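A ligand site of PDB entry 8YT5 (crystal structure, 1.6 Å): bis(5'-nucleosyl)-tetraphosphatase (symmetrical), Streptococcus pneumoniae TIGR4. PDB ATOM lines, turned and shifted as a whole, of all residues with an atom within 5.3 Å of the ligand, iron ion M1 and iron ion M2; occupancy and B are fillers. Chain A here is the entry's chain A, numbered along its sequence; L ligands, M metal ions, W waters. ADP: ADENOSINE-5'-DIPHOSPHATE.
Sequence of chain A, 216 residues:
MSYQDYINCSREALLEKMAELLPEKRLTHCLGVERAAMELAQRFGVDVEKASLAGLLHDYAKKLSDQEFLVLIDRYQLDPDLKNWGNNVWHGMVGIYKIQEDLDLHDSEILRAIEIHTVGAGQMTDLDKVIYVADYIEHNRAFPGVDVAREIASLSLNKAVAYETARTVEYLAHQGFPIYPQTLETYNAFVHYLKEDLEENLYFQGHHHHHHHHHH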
ATOM      1  N   ARG A  26       2.356  38.743 -28.180  1.00  0.00           N
ATOM      2  CA  ARG A  26       2.027  37.471 -28.817  1.00  0.00           C
ATOM      3  C   ARG A  26       2.008  37.599 -30.341  1.00  0.00           C
ATOM      4  O   ARG A  26       2.475  36.685 -31.038  1.00  0.00           O
ATOM      5  CB  ARG A  26       0.696  36.936 -28.269  1.00  0.00           C
ATOM      6  CG  ARG A  26       0.328  35.507 -28.704  1.00  0.00           C
ATOM      7  CD  ARG A  26       1.386  34.459 -28.396  1.00  0.00           C
ATOM      8  NE  ARG A  26       1.738  34.411 -26.980  1.00  0.00           N
ATOM      9  CZ  ARG A  26       2.604  33.556 -26.444  1.00  0.00           C
ATOM     10  NH1 ARG A  26       3.214  32.642 -27.194  1.00  0.00           N
ATOM     11  NH2 ARG A  26       2.865  33.614 -25.142  1.00  0.00           N
ATOM     12  N   HIS A  29       5.502  37.771 -31.495  1.00  0.00           N
ATOM     13  CA  HIS A  29       6.031  36.403 -31.497  1.00  0.00           C
ATOM     14  C   HIS A  29       5.614  35.660 -32.771  1.00  0.00           C
ATOM     15  O   HIS A  29       6.433  35.011 -33.405  1.00  0.00           O
ATOM     16  CB  HIS A  29       5.622  35.663 -30.228  1.00  0.00           C
ATOM     17  CG  HIS A  29       5.718  34.170 -30.320  1.00  0.00           C
ATOM     18  ND1 HIS A  29       6.919  33.499 -30.314  1.00  0.00           N
ATOM     19  CD2 HIS A  29       4.758  33.206 -30.399  1.00  0.00           C
ATOM     20  CE1 HIS A  29       6.699  32.194 -30.397  1.00  0.00           C
ATOM     21  NE2 HIS A  29       5.400  31.993 -30.439  1.00  0.00           N
ATOM     22  N   VAL A  33       7.911  33.963 -35.635  1.00  0.00           N
ATOM     23  CA  VAL A  33       7.799  32.568 -36.067  1.00  0.00           C
ATOM     24  C   VAL A  33       7.592  32.487 -37.593  1.00  0.00           C
ATOM     25  O   VAL A  33       8.160  31.616 -38.255  1.00  0.00           O
ATOM     26  CB  VAL A  33       6.724  31.806 -35.268  1.00  0.00           C
ATOM     27  CG1 VAL A  33       6.633  30.359 -35.706  1.00  0.00           C
ATOM     28  CG2 VAL A  33       7.023  31.852 -33.776  1.00  0.00           C
ATOM     29  N   HIS A  58       0.412  29.888 -35.861  1.00  0.00           N
ATOM     30  CA  HIS A  58       0.537  28.762 -34.920  1.00  0.00           C
ATOM     31  C   HIS A  58      -0.073  29.073 -33.545  1.00  0.00           C
ATOM     32  O   HIS A  58      -0.632  28.186 -32.909  1.00  0.00           O
ATOM     33  CB  HIS A  58       1.986  28.307 -34.792  1.00  0.00           C
ATOM     34  CG  HIS A  58       2.793  29.141 -33.863  1.00  0.00           C
ATOM     35  ND1 HIS A  58       3.175  30.420 -34.173  1.00  0.00           N
ATOM     36  CD2 HIS A  58       3.216  28.911 -32.598  1.00  0.00           C
ATOM     37  CE1 HIS A  58       3.843  30.939 -33.159  1.00  0.00           C
ATOM     38  NE2 HIS A  58       3.874  30.041 -32.180  1.00  0.00           N
ATOM     39  N   ASP A  59       0.021  30.334 -33.099  1.00  0.00           N
ATOM     40  CA  ASP A  59      -0.543  30.745 -31.812  1.00  0.00           C
ATOM     41  C   ASP A  59      -1.810  31.582 -31.946  1.00  0.00           C
ATOM     42  O   ASP A  59      -2.176  32.291 -31.013  1.00  0.00           O
ATOM     43  CB  ASP A  59       0.503  31.481 -30.950  1.00  0.00           C
ATOM     44  CG  ASP A  59       1.409  30.529 -30.166  1.00  0.00           C
ATOM     45  OD1 ASP A  59       1.060  29.351 -29.952  1.00  0.00           O
ATOM     46  OD2 ASP A  59       2.505  30.968 -29.765  1.00  0.00           O
ATOM     47  N   LYS A  62      -4.208  31.195 -29.004  1.00  0.00           N
ATOM     48  CA  LYS A  62      -3.583  31.251 -27.677  1.00  0.00           C
ATOM     49  C   LYS A  62      -4.482  31.851 -26.593  1.00  0.00           C
ATOM     50  O   LYS A  62      -4.364  31.486 -25.422  1.00  0.00           O
ATOM     51  CB  LYS A  62      -2.268  32.020 -27.750  1.00  0.00           C
ATOM     52  CG  LYS A  62      -1.407  31.992 -26.481  1.00  0.00           C
ATOM     53  CD  LYS A  62      -0.678  30.675 -26.269  1.00  0.00           C
ATOM     54  CE  LYS A  62       0.355  30.807 -25.156  1.00  0.00           C
ATOM     55  NZ  LYS A  62       1.265  29.621 -25.069  1.00  0.00           N
ATOM     56  N   TRP A  85      -6.674  18.564 -19.527  1.00  0.00           N
ATOM     57  CA  TRP A  85      -5.500  19.409 -19.706  1.00  0.00           C
ATOM     58  C   TRP A  85      -5.926  20.870 -19.780  1.00  0.00           C
ATOM     59  O   TRP A  85      -6.903  21.264 -19.149  1.00  0.00           O
ATOM     60  CB  TRP A  85      -4.695  18.929 -20.921  1.00  0.00           C
ATOM     61  CG  TRP A  85      -4.299  17.502 -20.739  1.00  0.00           C
ATOM     62  CD1 TRP A  85      -5.020  16.396 -21.080  1.00  0.00           C
ATOM     63  CD2 TRP A  85      -3.095  17.021 -20.111  1.00  0.00           C
ATOM     64  NE1 TRP A  85      -4.346  15.252 -20.730  1.00  0.00           N
ATOM     65  CE2 TRP A  85      -3.165  15.602 -20.125  1.00  0.00           C
ATOM     66  CE3 TRP A  85      -1.976  17.651 -19.559  1.00  0.00           C
ATOM     67  CZ2 TRP A  85      -2.147  14.796 -19.605  1.00  0.00           C
ATOM     68  CZ3 TRP A  85      -0.963  16.846 -19.031  1.00  0.00           C
ATOM     69  CH2 TRP A  85      -1.049  15.436 -19.056  1.00  0.00           C
ATOM     70  N   ASN A  88      -2.133  25.093 -22.742  1.00  0.00           N
ATOM     71  CA  ASN A  88      -0.871  24.631 -23.331  1.00  0.00           C
ATOM     72  C   ASN A  88      -1.085  23.547 -24.388  1.00  0.00           C
ATOM     73  O   ASN A  88      -0.576  23.659 -25.499  1.00  0.00           O
ATOM     74  CB  ASN A  88       0.108  24.120 -22.262  1.00  0.00           C
ATOM     75  CG  ASN A  88       0.621  25.239 -21.365  1.00  0.00           C
ATOM     76  OD1 ASN A  88       0.404  26.425 -21.614  1.00  0.00           O
ATOM     77  ND2 ASN A  88       1.325  24.846 -20.300  1.00  0.00           N
ATOM     78  N   VAL A  89      -1.870  22.540 -24.046  1.00  0.00           N
ATOM     79  CA  VAL A  89      -2.226  21.477 -24.980  1.00  0.00           C
ATOM     80  C   VAL A  89      -3.251  21.973 -25.994  1.00  0.00           C
ATOM     81  O   VAL A  89      -3.132  21.719 -27.195  1.00  0.00           O
ATOM     82  CB  VAL A  89      -2.748  20.228 -24.217  1.00  0.00           C
ATOM     83  CG1 VAL A  89      -3.250  19.171 -25.183  1.00  0.00           C
ATOM     84  CG2 VAL A  89      -1.652  19.628 -23.350  1.00  0.00           C
ATOM     85  N   HIS A  91      -4.266  24.973 -27.289  1.00  0.00           N
ATOM     86  CA  HIS A  91      -4.259  26.093 -28.253  1.00  0.00           C
ATOM     87  C   HIS A  91      -3.808  25.655 -29.632  1.00  0.00           C
ATOM     88  O   HIS A  91      -4.261  26.184 -30.637  1.00  0.00           O
ATOM     89  CB  HIS A  91      -3.516  27.334 -27.746  1.00  0.00           C
ATOM     90  CG  HIS A  91      -2.026  27.200 -27.718  1.00  0.00           C
ATOM     91  ND1 HIS A  91      -1.367  26.456 -26.766  1.00  0.00           N
ATOM     92  CD2 HIS A  91      -1.074  27.716 -28.523  1.00  0.00           C
ATOM     93  CE1 HIS A  91      -0.069  26.512 -26.993  1.00  0.00           C
ATOM     94  NE2 HIS A  91       0.140  27.282 -28.046  1.00  0.00           N
ATOM     95  N   HIS A 117       2.295  21.819 -32.811  1.00  0.00           N
ATOM     96  CA  HIS A 117       3.445  22.728 -32.645  1.00  0.00           C
ATOM     97  C   HIS A 117       3.970  22.785 -31.214  1.00  0.00           C
ATOM     98  O   HIS A 117       5.126  23.143 -31.004  1.00  0.00           O
ATOM     99  CB  HIS A 117       3.132  24.133 -33.162  1.00  0.00           C
ATOM    100  CG  HIS A 117       2.399  24.988 -32.164  1.00  0.00           C
ATOM    101  ND1 HIS A 117       1.030  25.097 -32.162  1.00  0.00           N
ATOM    102  CD2 HIS A 117       2.852  25.766 -31.154  1.00  0.00           C
ATOM    103  CE1 HIS A 117       0.663  25.906 -31.180  1.00  0.00           C
ATOM    104  NE2 HIS A 117       1.745  26.328 -30.561  1.00  0.00           N
ATOM    105  N   THR A 118       3.134  22.439 -30.236  1.00  0.00           N
ATOM    106  CA  THR A 118       3.548  22.462 -28.836  1.00  0.00           C
ATOM    107  C   THR A 118       4.091  21.109 -28.405  1.00  0.00           C
ATOM    108  O   THR A 118       5.177  21.037 -27.807  1.00  0.00           O
ATOM    109  CB  THR A 118       2.372  22.822 -27.912  1.00  0.00           C
ATOM    110  OG1 THR A 118       1.750  24.036 -28.343  1.00  0.00           O
ATOM    111  CG2 THR A 118       2.826  22.939 -26.449  1.00  0.00           C
ATOM    112  N   VAL A 119       3.366  20.038 -28.718  1.00  0.00           N
ATOM    113  CA  VAL A 119       3.680  18.719 -28.184  1.00  0.00           C
ATOM    114  C   VAL A 119       4.466  17.807 -29.132  1.00  0.00           C
ATOM    115  O   VAL A 119       4.997  16.777 -28.704  1.00  0.00           O
ATOM    116  CB  VAL A 119       2.407  17.997 -27.677  1.00  0.00           C
ATOM    117  CG1 VAL A 119       1.827  18.745 -26.491  1.00  0.00           C
ATOM    118  CG2 VAL A 119       1.375  17.829 -28.785  1.00  0.00           C
ATOM    119  N   ASP A 135       9.081  28.138 -33.643  1.00  0.00           N
ATOM    120  CA  ASP A 135       8.420  28.648 -32.449  1.00  0.00           C
ATOM    121  C   ASP A 135       9.429  28.898 -31.327  1.00  0.00           C
ATOM    122  O   ASP A 135       9.349  29.893 -30.598  1.00  0.00           O
ATOM    123  CB  ASP A 135       7.367  27.616 -32.024  1.00  0.00           C
ATOM    124  CG  ASP A 135       6.514  28.060 -30.872  1.00  0.00           C
ATOM    125  OD1 ASP A 135       6.260  29.276 -30.673  1.00  0.00           O
ATOM    126  OD2 ASP A 135       6.026  27.156 -30.180  1.00  0.00           O
ATOM    127  N   ARG A 141      12.586  35.493 -28.913  1.00  0.00           N
ATOM    128  CA  ARG A 141      12.838  34.601 -27.762  1.00  0.00           C
ATOM    129  C   ARG A 141      14.171  34.930 -27.108  1.00  0.00           C
ATOM    130  O   ARG A 141      15.152  35.192 -27.788  1.00  0.00           O
ATOM    131  CB  ARG A 141      12.861  33.138 -28.198  1.00  0.00           C
ATOM    132  CG  ARG A 141      11.611  32.583 -28.873  1.00  0.00           C
ATOM    133  CD  ARG A 141      10.372  32.737 -28.028  1.00  0.00           C
ATOM    134  NE  ARG A 141      10.374  31.952 -26.806  1.00  0.00           N
ATOM    135  CZ  ARG A 141       9.916  30.711 -26.712  1.00  0.00           C
ATOM    136  NH1 ARG A 141       9.436  30.101 -27.790  1.00  0.00           N
ATOM    137  NH2 ARG A 141       9.907  30.078 -25.559  1.00  0.00           N
ATOM    138  N   GLU A 164      15.008  20.744 -28.409  1.00  0.00           N
ATOM    139  CA  GLU A 164      13.857  21.470 -27.870  1.00  0.00           C
ATOM    140  C   GLU A 164      13.017  20.560 -26.970  1.00  0.00           C
ATOM    141  O   GLU A 164      12.605  20.969 -25.884  1.00  0.00           O
ATOM    142  CB  GLU A 164      12.991  22.057 -28.983  1.00  0.00           C
ATOM    143  CG  GLU A 164      11.769  22.771 -28.428  1.00  0.00           C
ATOM    144  CD  GLU A 164      10.863  23.342 -29.494  1.00  0.00           C
ATOM    145  OE1 GLU A 164      11.286  23.409 -30.666  1.00  0.00           O
ATOM    146  OE2 GLU A 164       9.737  23.748 -29.145  1.00  0.00           O
ATOM    147  N   THR A 168      12.316  20.888 -22.973  1.00  0.00           N
ATOM    148  CA  THR A 168      10.948  21.072 -22.529  1.00  0.00           C
ATOM    149  C   THR A 168      10.533  20.046 -21.473  1.00  0.00           C
ATOM    150  O   THR A 168       9.959  20.414 -20.447  1.00  0.00           O
ATOM    151  CB  THR A 168       9.995  21.078 -23.723  1.00  0.00           C
ATOM    152  OG1 THR A 168      10.283  22.253 -24.495  1.00  0.00           O
ATOM    153  CG2 THR A 168       8.540  21.139 -23.263  1.00  0.00           C
ATOM    154  N   LEU A 172       9.634  21.065 -17.664  1.00  0.00           N
ATOM    155  CA  LEU A 172       8.338  20.754 -17.069  1.00  0.00           C
ATOM    156  C   LEU A 172       8.517  19.959 -15.784  1.00  0.00           C
ATOM    157  O   LEU A 172       7.861  20.253 -14.778  1.00  0.00           O
ATOM    158  CB  LEU A 172       7.447  20.017 -18.059  1.00  0.00           C
ATOM    159  CG  LEU A 172       6.985  20.846 -19.252  1.00  0.00           C
ATOM    160  CD1 LEU A 172       6.390  19.952 -20.315  1.00  0.00           C
ATOM    161  CD2 LEU A 172       6.008  21.939 -18.841  1.00  0.00           C
ATOM    162  N   PRO A 178       2.431  18.804 -15.023  1.00  0.00           N
ATOM    163  CA  PRO A 178       2.076  17.600 -15.777  1.00  0.00           C
ATOM    164  C   PRO A 178       2.591  17.673 -17.212  1.00  0.00           C
ATOM    165  O   PRO A 178       2.656  18.767 -17.807  1.00  0.00           O
ATOM    166  CB  PRO A 178       0.543  17.611 -15.761  1.00  0.00           C
ATOM    167  CG  PRO A 178       0.168  18.466 -14.599  1.00  0.00           C
ATOM    168  CD  PRO A 178       1.233  19.514 -14.535  1.00  0.00           C
ATOM    169  N   ILE A 179       2.993  16.526 -17.750  1.00  0.00           N
ATOM    170  CA  ILE A 179       3.526  16.448 -19.100  1.00  0.00           C
ATOM    171  C   ILE A 179       2.554  15.666 -19.971  1.00  0.00           C
ATOM    172  O   ILE A 179       2.321  14.479 -19.743  1.00  0.00           O
ATOM    173  CB  ILE A 179       4.927  15.791 -19.113  1.00  0.00           C
ATOM    174  CG1 ILE A 179       5.911  16.642 -18.300  1.00  0.00           C
ATOM    175  CG2 ILE A 179       5.426  15.588 -20.543  1.00  0.00           C
ATOM    176  CD1 ILE A 179       7.184  15.913 -17.901  1.00  0.00           C
ATOM    177  N   TYR A 180       1.989  16.347 -20.966  1.00  0.00           N
ATOM    178  CA  TYR A 180       1.089  15.683 -21.898  1.00  0.00           C
ATOM    179  C   TYR A 180       1.827  14.530 -22.569  1.00  0.00           C
ATOM    180  O   TYR A 180       2.931  14.719 -23.059  1.00  0.00           O
ATOM    181  CB  TYR A 180       0.582  16.669 -22.944  1.00  0.00           C
ATOM    182  CG  TYR A 180      -0.535  16.130 -23.786  1.00  0.00           C
ATOM    183  CD1 TYR A 180      -1.786  15.869 -23.227  1.00  0.00           C
ATOM    184  CD2 TYR A 180      -0.349  15.879 -25.146  1.00  0.00           C
ATOM    185  CE1 TYR A 180      -2.824  15.362 -24.000  1.00  0.00           C
ATOM    186  CE2 TYR A 180      -1.387  15.379 -25.931  1.00  0.00           C
ATOM    187  CZ  TYR A 180      -2.617  15.130 -25.348  1.00  0.00           C
ATOM    188  OH  TYR A 180      -3.648  14.629 -26.118  1.00  0.00           O
ATOM    189  N   THR A 183       4.046  14.497 -25.853  1.00  0.00           N
ATOM    190  CA  THR A 183       5.397  15.041 -25.751  1.00  0.00           C
ATOM    191  C   THR A 183       6.457  13.978 -25.500  1.00  0.00           C
ATOM    192  O   THR A 183       7.557  14.038 -26.039  1.00  0.00           O
ATOM    193  CB  THR A 183       5.452  16.155 -24.690  1.00  0.00           C
ATOM    194  OG1 THR A 183       4.640  17.239 -25.168  1.00  0.00           O
ATOM    195  CG2 THR A 183       6.863  16.649 -24.429  1.00  0.00           C
HETATM  196  PB  ADP L   1       4.147  29.296 -27.028  1.00  0.00           P
HETATM  197  O1B ADP L   1       4.329  29.816 -25.618  1.00  0.00           O
HETATM  198  O2B ADP L   1       4.808  30.187 -28.049  1.00  0.00           O
HETATM  199  O3B ADP L   1       2.695  29.008 -27.393  1.00  0.00           O
HETATM  200  PA  ADP L   1       4.421  26.386 -27.004  1.00  0.00           P
HETATM  201  O1A ADP L   1       5.470  25.432 -27.538  1.00  0.00           O
HETATM  202  O2A ADP L   1       3.060  26.261 -27.624  1.00  0.00           O
HETATM  203  O3A ADP L   1       4.982  27.905 -27.132  1.00  0.00           O
HETATM  204  O5' ADP L   1       4.297  26.057 -25.444  1.00  0.00           O
HETATM  205  C5' ADP L   1       3.421  26.788 -24.594  1.00  0.00           C
HETATM  206  C4' ADP L   1       3.559  26.221 -23.179  1.00  0.00           C
HETATM  207  O4' ADP L   1       3.194  24.823 -23.188  1.00  0.00           O
HETATM  208  C3' ADP L   1       4.965  26.368 -22.627  1.00  0.00           C
HETATM  209  O3' ADP L   1       4.890  26.916 -21.297  1.00  0.00           O
HETATM  210  C2' ADP L   1       5.397  24.921 -22.587  1.00  0.00           C
HETATM  211  O2' ADP L   1       6.245  24.700 -21.485  1.00  0.00           O
HETATM  212  C1' ADP L   1       4.107  24.149 -22.369  1.00  0.00           C
HETATM  213  N9  ADP L   1       4.194  22.734 -22.734  1.00  0.00           N
HETATM  214  C8  ADP L   1       4.936  22.221 -23.724  1.00  0.00           C
HETATM  215  N7  ADP L   1       4.790  20.885 -23.758  1.00  0.00           N
HETATM  216  C5  ADP L   1       3.949  20.547 -22.784  1.00  0.00           C
HETATM  217  C6  ADP L   1       3.379  19.304 -22.263  1.00  0.00           C
HETATM  218  N6  ADP L   1       3.669  18.108 -22.807  1.00  0.00           N
HETATM  219  N1  ADP L   1       2.544  19.387 -21.219  1.00  0.00           N
HETATM  220  C2  ADP L   1       2.229  20.558 -20.640  1.00  0.00           C
HETATM  221  N3  ADP L   1       2.712  21.729 -21.067  1.00  0.00           N
HETATM  222  C4  ADP L   1       3.565  21.771 -22.112  1.00  0.00           C
HETATM  223 FE    FE M   1       2.053  27.803 -28.904  1.00  0.00          FE
HETATM  224 FE    FE M   2       4.498  30.088 -30.109  1.00  0.00          FE
HETATM  225  O   HOH W   1       7.011  32.081 -26.910  1.00  0.00           O
HETATM  226  O   HOH W   2       4.541  25.392 -18.699  1.00  0.00           O
HETATM  227  O   HOH W   3       5.385  31.803 -24.220  1.00  0.00           O
HETATM  228  O   HOH W   4       7.159  24.518 -29.791  1.00  0.00           O
HETATM  229  O   HOH W   5       6.218  19.638 -25.752  1.00  0.00           O
HETATM  230  O   HOH W   6       3.473  30.258 -22.709  1.00  0.00           O
HETATM  231  O   HOH W   7       6.799  28.971 -24.595  1.00  0.00           O
HETATM  232  O   HOH W   8       2.583  23.561 -18.110  1.00  0.00           O
HETATM  233  O   HOH W   9       8.160  27.138 -27.992  1.00  0.00           O
HETATM  234  O   HOH W  10       1.306  21.139 -17.620  1.00  0.00           O
HETATM  235  O   HOH W  11       3.761  28.339 -29.726  1.00  0.00           O
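OG1 of Thr 118 sits close to O2A of the ligand (2.7 Å).
OG1 of Thr 183 is in hydrogen-bond range of N6 of the ligand, 2.7 Å away.
The side-chain amino group (NZ) of Lys 62 is in salt-bridge range of an oxygen (O1B) of the ligand (3.1 Å).
The guanidinium group of Arg 26 lies within salt-bridge range of an oxygen (O1B) of the ligand (3.4 Å).
The backbone NH (N) of Tyr 180 lies within hydrogen-bond range of a nitrogen (N1) of the ligand (3.1 Å).
N6 of the ligand sits close to O of Tyr 180, at 3.5 Å.
O4' of the ligand lies close to ND2 of Asn 88 (3.4 Å).
O of Asp 135 sits at hydrogen-bond distance from NH1 of Arg 141.
The guanidinium group of Arg 26 sits close to the side-chain carboxylate of Asp 59 (3.1 Å).
O of Asn 88 lies within hydrogen-bond range of ND1 of His 91 (3.2 Å).
NE2 of His 117 lies close to OG1 of Thr 118 (3.2 Å).
The side-chain hydroxyl (OG1) of Thr 168 is in hydrogen-bond range of the backbone carbonyl oxygen (O) of Glu 164, 3.0 Å away.
The backbone carbonyl oxygen of Pro 178 sits close to a nitrogen (N1) of the ligand (3.5 Å).
Residues that only touch the ligand: Thr 168 (3.8 Å), Leu 172 (3.5 Å) and Ile 179 (3.8 Å).
Hydrophobic or aromatic side chains that line the ligand: His 29, His 91, His 117, Leu 172, Ile 179 and Tyr 180.
Within 4 Å of the ligand: Arg 26, His 29, Asp 59, Lys 62, Asn 88, His 91, His 117, Thr 118, Asp 135, Thr 168, Leu 172, Pro 178, Ile 179, Tyr 180 and Thr 183.
Thr 118 touches iron ion M1.
Within 4 Å of iron ion M1: Asp 59, His 91, His 117 and Thr 118.
The nearest printed residue that does not touch iron ion M1 is His 58 (4.03 Å).
Four residues have an atom within 4 Å of iron ion M2: His 29, His 58, Asp 59 and Asp 135.
Water W11 is bound to iron ion M1 (2.0 Å).
An oxygen (O3B) of the ligand binds iron ion M1 (2.0 Å).
Iron ion M1 is bound by OD1 of Asp 59, at 2.1 Å.
NE2 of His 91 is bound to iron ion M1.
NE2 of His 117 is bound to iron ion M1 (2.2 Å).
O2A of the ligand binds iron ion M1, at 2.2 Å.
Water W11 binds iron ion M2 (1.9 Å).
OD1 of Asp 135 binds iron ion M2, at 2.0 Å.
O2B of the ligand is bound to iron ion M2 (2.1 Å).
NE2 of His 29 binds iron ion M2, at 2.1 Å.
A ring nitrogen (NE2) of His 58 is bound to iron ion M2, 2.2 Å away.
OD2 of Asp 59 binds iron ion M2.
Iron ion M2 has six donor atoms within binding distance.
Water W11 lies within hydrogen-bond range of the side-chain carboxylate of Asp 135 and an oxygen (O3A) of the ligand.
Water W3 bridges an oxygen (O1B) of the ligand (2.6 Å) and the guanidinium group (NH2) of Arg 26 (3.2 Å).
Water W5 lies within hydrogen-bond range of O of Thr 118 (2.7 Å), N7 of the ligand (2.8 Å) and OG1 of Thr 183 (2.9 Å).
Water W7 lies within hydrogen-bond range of an oxygen (O1B) of the ligand (2.8 Å) and the guanidinium group (NH2) of Arg 141 (3.4 Å).
Water W9 lies within hydrogen-bond range of OD2 of Asp 135, O1A of the ligand and NH1 of Arg 141.
Water W8 bridges the side-chain amide nitrogen (ND2) of Asn 88 (2.8 Å) and a nitrogen (N3) of the ligand (3.5 Å).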
